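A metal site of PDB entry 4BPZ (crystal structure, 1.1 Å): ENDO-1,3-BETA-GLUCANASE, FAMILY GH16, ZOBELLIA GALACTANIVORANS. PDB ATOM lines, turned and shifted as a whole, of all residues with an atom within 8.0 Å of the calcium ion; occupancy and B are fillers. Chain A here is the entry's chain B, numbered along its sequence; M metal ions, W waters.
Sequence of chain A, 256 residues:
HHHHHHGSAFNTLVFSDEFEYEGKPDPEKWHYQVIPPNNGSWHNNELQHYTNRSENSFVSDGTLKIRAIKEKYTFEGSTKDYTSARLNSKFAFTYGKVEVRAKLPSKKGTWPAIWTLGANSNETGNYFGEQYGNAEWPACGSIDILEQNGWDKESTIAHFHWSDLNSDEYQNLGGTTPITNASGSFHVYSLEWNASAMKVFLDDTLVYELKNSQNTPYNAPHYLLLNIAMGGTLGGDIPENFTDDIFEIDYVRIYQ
NE of Arg 253 is in salt-bridge range of OE2 of Glu 18 (2.8 Å).
The guanidinium group of Arg 101 is in salt-bridge range of the side-chain carboxylate of Asp 250.
Along chain A the residues within 4 Å of the calcium ion span positions 18 to 250.
The nearest printed residue that does not touch the calcium ion is Glu 20 (4.4 Å).
O of Glu 18 binds the calcium ion (2.2 Å).
The calcium ion is bound by O of Gly 62 (2.3 Å).
Water W1 is bound to the calcium ion, 2.4 Å away.
The calcium ion is bound by the backbone carbonyl oxygen (O) of Asp 250, at 2.4 Å.
OD1 of Asp 250 binds the calcium ion (2.4 Å).
Water W2 is bound to the calcium ion (2.4 Å).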
ATOM      1  N   ASP A  17      -6.832  31.008   2.701  1.00  0.00           N
ATOM      2  CA  ASP A  17      -5.822  30.473   1.788  1.00  0.00           C
ATOM      3  C   ASP A  17      -6.631  29.599   0.787  1.00  0.00           C
ATOM      4  O   ASP A  17      -7.292  28.624   1.210  1.00  0.00           O
ATOM      5  CB  ASP A  17      -4.744  29.712   2.523  1.00  0.00           C
ATOM      6  CG  ASP A  17      -3.506  29.531   1.681  1.00  0.00           C
ATOM      7  OD1 ASP A  17      -3.623  29.613   0.405  1.00  0.00           O
ATOM      8  OD2 ASP A  17      -2.449  29.203   2.288  1.00  0.00           O
ATOM      9  N   GLU A  18      -6.474  29.941  -0.494  1.00  0.00           N
ATOM     10  CA  GLU A  18      -7.110  29.152  -1.606  1.00  0.00           C
ATOM     11  C   GLU A  18      -6.172  28.117  -2.106  1.00  0.00           C
ATOM     12  O   GLU A  18      -6.607  27.180  -2.924  1.00  0.00           O
ATOM     13  CB  GLU A  18      -7.583  30.082  -2.736  1.00  0.00           C
ATOM     14  CG  GLU A  18      -8.522  31.188  -2.229  1.00  0.00           C
ATOM     15  CD  GLU A  18      -9.852  30.615  -1.756  1.00  0.00           C
ATOM     16  OE1 GLU A  18     -10.411  29.669  -2.391  1.00  0.00           O
ATOM     17  OE2 GLU A  18     -10.490  31.222  -0.896  1.00  0.00           O
ATOM     18  N   PHE A  19      -4.955  28.207  -1.632  1.00  0.00           N
ATOM     19  CA  PHE A  19      -3.895  27.145  -1.907  1.00  0.00           C
ATOM     20  C   PHE A  19      -3.664  27.067  -3.432  1.00  0.00           C
ATOM     21  O   PHE A  19      -3.598  25.994  -4.007  1.00  0.00           O
ATOM     22  CB  PHE A  19      -4.326  25.775  -1.322  1.00  0.00           C
ATOM     23  CG  PHE A  19      -4.377  25.798   0.142  1.00  0.00           C
ATOM     24  CD1 PHE A  19      -3.220  26.149   0.852  1.00  0.00           C
ATOM     25  CD2 PHE A  19      -5.580  25.593   0.852  1.00  0.00           C
ATOM     26  CE1 PHE A  19      -3.200  26.213   2.249  1.00  0.00           C
ATOM     27  CE2 PHE A  19      -5.544  25.629   2.283  1.00  0.00           C
ATOM     28  CZ  PHE A  19      -4.400  25.978   2.995  1.00  0.00           C
ATOM     29  N   GLU A  20      -3.632  28.241  -4.073  1.00  0.00           N
ATOM     30  CA  GLU A  20      -3.478  28.262  -5.531  1.00  0.00           C
ATOM     31  C   GLU A  20      -2.055  28.704  -5.838  1.00  0.00           C
ATOM     32  O   GLU A  20      -1.784  29.592  -6.747  1.00  0.00           O
ATOM     33  CB  GLU A  20      -4.524  29.188  -6.186  1.00  0.00           C
ATOM     34  CG  GLU A  20      -5.976  28.704  -6.067  1.00  0.00           C
ATOM     35  CD  GLU A  20      -7.053  29.782  -6.390  1.00  0.00           C
ATOM     36  OE1 GLU A  20      -6.711  30.905  -6.831  1.00  0.00           O
ATOM     37  OE2 GLU A  20      -8.280  29.520  -6.205  1.00  0.00           O
ATOM     38  N   TYR A  21      -1.099  28.049  -5.193  1.00  0.00           N
ATOM     39  CA  TYR A  21       0.339  28.159  -5.415  1.00  0.00           C
ATOM     40  C   TYR A  21       0.969  26.781  -5.383  1.00  0.00           C
ATOM     41  O   TYR A  21       0.336  25.771  -5.043  1.00  0.00           O
ATOM     42  CB  TYR A  21       1.012  29.115  -4.381  1.00  0.00           C
ATOM     43  CG  TYR A  21       0.630  28.841  -2.946  1.00  0.00           C
ATOM     44  CD1 TYR A  21      -0.528  29.371  -2.418  1.00  0.00           C
ATOM     45  CD2 TYR A  21       1.468  28.067  -2.141  1.00  0.00           C
ATOM     46  CE1 TYR A  21      -0.910  29.109  -1.119  1.00  0.00           C
ATOM     47  CE2 TYR A  21       1.143  27.802  -0.849  1.00  0.00           C
ATOM     48  CZ  TYR A  21      -0.039  28.339  -0.325  1.00  0.00           C
ATOM     49  OH  TYR A  21      -0.426  28.035   0.990  1.00  0.00           O
ATOM     50  N   VAL A  59       1.607  22.046  -1.197  1.00  0.00           N
ATOM     51  CA  VAL A  59       0.452  22.664  -1.856  1.00  0.00           C
ATOM     52  C   VAL A  59       0.667  22.502  -3.365  1.00  0.00           C
ATOM     53  O   VAL A  59       1.766  22.771  -3.882  1.00  0.00           O
ATOM     54  CB  VAL A  59       0.366  24.181  -1.481  1.00  0.00           C
ATOM     55  CG1 VAL A  59      -0.802  24.837  -2.145  1.00  0.00           C
ATOM     56  CG2 VAL A  59       0.253  24.377   0.020  1.00  0.00           C
ATOM     57  N   SER A  60      -0.369  22.077  -4.106  1.00  0.00           N
ATOM     58  CA  SER A  60      -0.152  21.875  -5.543  1.00  0.00           C
ATOM     59  C   SER A  60      -1.556  21.630  -6.112  1.00  0.00           C
ATOM     60  O   SER A  60      -2.487  21.159  -5.418  1.00  0.00           O
ATOM     61  CB  SER A  60       0.733  20.648  -5.842  1.00  0.00           C
ATOM     62  OG  SER A  60       0.159  19.480  -5.203  1.00  0.00           O
ATOM     63  N   ASP A  61      -1.683  21.993  -7.389  1.00  0.00           N
ATOM     64  CA  ASP A  61      -2.939  21.871  -8.107  1.00  0.00           C
ATOM     65  C   ASP A  61      -4.162  22.359  -7.370  1.00  0.00           C
ATOM     66  O   ASP A  61      -5.223  21.689  -7.420  1.00  0.00           O
ATOM     67  CB  ASP A  61      -3.121  20.419  -8.523  1.00  0.00           C
ATOM     68  CG  ASP A  61      -1.913  19.898  -9.251  1.00  0.00           C
ATOM     69  OD1 ASP A  61      -1.433  20.663 -10.131  1.00  0.00           O
ATOM     70  OD2 ASP A  61      -1.446  18.806  -8.869  1.00  0.00           O
ATOM     71  N   GLY A  62      -3.993  23.494  -6.701  1.00  0.00           N
ATOM     72  CA  GLY A  62      -5.098  24.190  -5.989  1.00  0.00           C
ATOM     73  C   GLY A  62      -5.516  23.639  -4.625  1.00  0.00           C
ATOM     74  O   GLY A  62      -6.450  24.139  -4.072  1.00  0.00           O
ATOM     75  N   THR A  63      -4.787  22.702  -4.081  1.00  0.00           N
ATOM     76  CA  THR A  63      -5.103  22.226  -2.733  1.00  0.00           C
ATOM     77  C   THR A  63      -3.859  22.032  -1.896  1.00  0.00           C
ATOM     78  O   THR A  63      -2.771  21.723  -2.351  1.00  0.00           O
ATOM     79  CB  THR A  63      -5.871  20.910  -2.829  1.00  0.00           C
ATOM     80  OG1 THR A  63      -4.984  19.877  -3.279  1.00  0.00           O
ATOM     81  CG2 THR A  63      -7.098  20.996  -3.653  1.00  0.00           C
ATOM     82  N   LEU A  64      -4.050  22.138  -0.576  1.00  0.00           N
ATOM     83  CA  LEU A  64      -3.072  21.733   0.464  1.00  0.00           C
ATOM     84  C   LEU A  64      -3.281  20.217   0.746  1.00  0.00           C
ATOM     85  O   LEU A  64      -4.413  19.716   0.862  1.00  0.00           O
ATOM     86  CB  LEU A  64      -3.350  22.484   1.807  1.00  0.00           C
ATOM     87  CG  LEU A  64      -2.651  21.957   3.038  1.00  0.00           C
ATOM     88  CD1 LEU A  64      -1.175  22.191   2.946  1.00  0.00           C
ATOM     89  CD2 LEU A  64      -3.279  22.743   4.239  1.00  0.00           C
ATOM     90  N   ARG A 101     -12.964  23.508   3.091  1.00  0.00           N
ATOM     91  CA  ARG A 101     -13.495  22.520   2.109  1.00  0.00           C
ATOM     92  C   ARG A 101     -12.392  21.472   1.992  1.00  0.00           C
ATOM     93  O   ARG A 101     -11.236  21.846   1.716  1.00  0.00           O
ATOM     94  CB  ARG A 101     -13.733  23.222   0.789  1.00  0.00           C
ATOM     95  CG  ARG A 101     -14.377  22.260  -0.249  1.00  0.00           C
ATOM     96  CD  ARG A 101     -14.831  23.003  -1.524  1.00  0.00           C
ATOM     97  NE  ARG A 101     -15.676  22.162  -2.397  1.00  0.00           N
ATOM     98  CZ  ARG A 101     -15.269  21.659  -3.553  1.00  0.00           C
ATOM     99  NH1 ARG A 101     -14.041  21.934  -3.924  1.00  0.00           N
ATOM    100  NH2 ARG A 101     -16.050  20.865  -4.286  1.00  0.00           N
ATOM    101  N   PHE A 186     -15.306  16.350  -1.845  1.00  0.00           N
ATOM    102  CA  PHE A 186     -15.063  17.451  -0.951  1.00  0.00           C
ATOM    103  C   PHE A 186     -16.353  17.809  -0.203  1.00  0.00           C
ATOM    104  O   PHE A 186     -17.453  17.655  -0.723  1.00  0.00           O
ATOM    105  CB  PHE A 186     -14.687  18.726  -1.762  1.00  0.00           C
ATOM    106  CG  PHE A 186     -13.234  18.770  -2.193  1.00  0.00           C
ATOM    107  CD1 PHE A 186     -12.213  19.008  -1.284  1.00  0.00           C
ATOM    108  CD2 PHE A 186     -12.898  18.582  -3.541  1.00  0.00           C
ATOM    109  CE1 PHE A 186     -10.869  19.046  -1.635  1.00  0.00           C
ATOM    110  CE2 PHE A 186     -11.544  18.632  -3.907  1.00  0.00           C
ATOM    111  CZ  PHE A 186     -10.526  18.890  -2.998  1.00  0.00           C
ATOM    112  N   ILE A 249      -7.036  19.762   1.474  1.00  0.00           N
ATOM    113  CA  ILE A 249      -7.850  20.928   1.756  1.00  0.00           C
ATOM    114  C   ILE A 249      -7.819  21.948   0.610  1.00  0.00           C
ATOM    115  O   ILE A 249      -6.793  22.397   0.210  1.00  0.00           O
ATOM    116  CB  ILE A 249      -7.279  21.595   3.006  1.00  0.00           C
ATOM    117  CG1 ILE A 249      -7.499  20.599   4.215  1.00  0.00           C
ATOM    118  CG2 ILE A 249      -7.980  22.907   3.364  1.00  0.00           C
ATOM    119  CD1 ILE A 249      -6.744  21.029   5.411  1.00  0.00           C
ATOM    120  N   ASP A 250      -8.985  22.159   0.033  1.00  0.00           N
ATOM    121  CA  ASP A 250      -9.160  23.110  -1.111  1.00  0.00           C
ATOM    122  C   ASP A 250      -8.959  24.524  -0.649  1.00  0.00           C
ATOM    123  O   ASP A 250      -8.322  25.358  -1.331  1.00  0.00           O
ATOM    124  CB  ASP A 250     -10.582  22.833  -1.784  1.00  0.00           C
ATOM    125  CG  ASP A 250     -10.803  23.658  -3.014  1.00  0.00           C
ATOM    126  OD1 ASP A 250      -9.790  24.058  -3.655  1.00  0.00           O
ATOM    127  OD2 ASP A 250     -12.017  23.869  -3.327  1.00  0.00           O
ATOM    128  N   TYR A 251      -9.529  24.904   0.510  1.00  0.00           N
ATOM    129  CA  TYR A 251      -9.436  26.283   0.989  1.00  0.00           C
ATOM    130  C   TYR A 251      -9.811  26.343   2.443  1.00  0.00           C
ATOM    131  O   TYR A 251     -10.471  25.447   3.000  1.00  0.00           O
ATOM    132  CB  TYR A 251     -10.349  27.319   0.207  1.00  0.00           C
ATOM    133  CG  TYR A 251     -11.841  27.065   0.173  1.00  0.00           C
ATOM    134  CD1 TYR A 251     -12.661  27.279   1.340  1.00  0.00           C
ATOM    135  CD2 TYR A 251     -12.435  26.625  -0.968  1.00  0.00           C
ATOM    136  CE1 TYR A 251     -14.027  27.083   1.230  1.00  0.00           C
ATOM    137  CE2 TYR A 251     -13.759  26.374  -1.040  1.00  0.00           C
ATOM    138  CZ  TYR A 251     -14.576  26.640   0.047  1.00  0.00           C
ATOM    139  OH  TYR A 251     -15.888  26.399   0.073  1.00  0.00           O
ATOM    140  N   VAL A 252      -9.237  27.341   3.083  1.00  0.00           N
ATOM    141  CA  VAL A 252      -9.728  27.851   4.365  1.00  0.00           C
ATOM    142  C   VAL A 252     -10.162  29.288   4.198  1.00  0.00           C
ATOM    143  O   VAL A 252      -9.396  30.088   3.633  1.00  0.00           O
ATOM    144  CB  VAL A 252      -8.537  27.879   5.401  1.00  0.00           C
ATOM    145  CG1 VAL A 252      -8.909  28.476   6.744  1.00  0.00           C
ATOM    146  CG2 VAL A 252      -8.089  26.384   5.559  1.00  0.00           C
ATOM    147  N   ARG A 253     -11.346  29.623   4.709  1.00  0.00           N
ATOM    148  CA  ARG A 253     -11.866  31.027   4.611  1.00  0.00           C
ATOM    149  C   ARG A 253     -12.388  31.360   6.013  1.00  0.00           C
ATOM    150  O   ARG A 253     -13.103  30.546   6.614  1.00  0.00           O
ATOM    151  CB  ARG A 253     -12.990  31.150   3.543  1.00  0.00           C
ATOM    152  CG  ARG A 253     -12.473  30.958   2.142  1.00  0.00           C
ATOM    153  CD  ARG A 253     -13.607  30.816   1.148  1.00  0.00           C
ATOM    154  NE  ARG A 253     -13.109  30.509  -0.193  1.00  0.00           N
ATOM    155  CZ  ARG A 253     -13.864  30.046  -1.168  1.00  0.00           C
ATOM    156  NH1 ARG A 253     -15.174  29.914  -0.979  1.00  0.00           N
ATOM    157  NH2 ARG A 253     -13.280  29.718  -2.336  1.00  0.00           N
HETATM  158 CA    CA M   1      -8.050  25.690  -3.665  1.00  0.00          CA
HETATM  159  O   HOH W   1      -8.083  25.759  -6.018  1.00  0.00           O
HETATM  160  O   HOH W   2      -9.886  27.296  -3.689  1.00  0.00           O
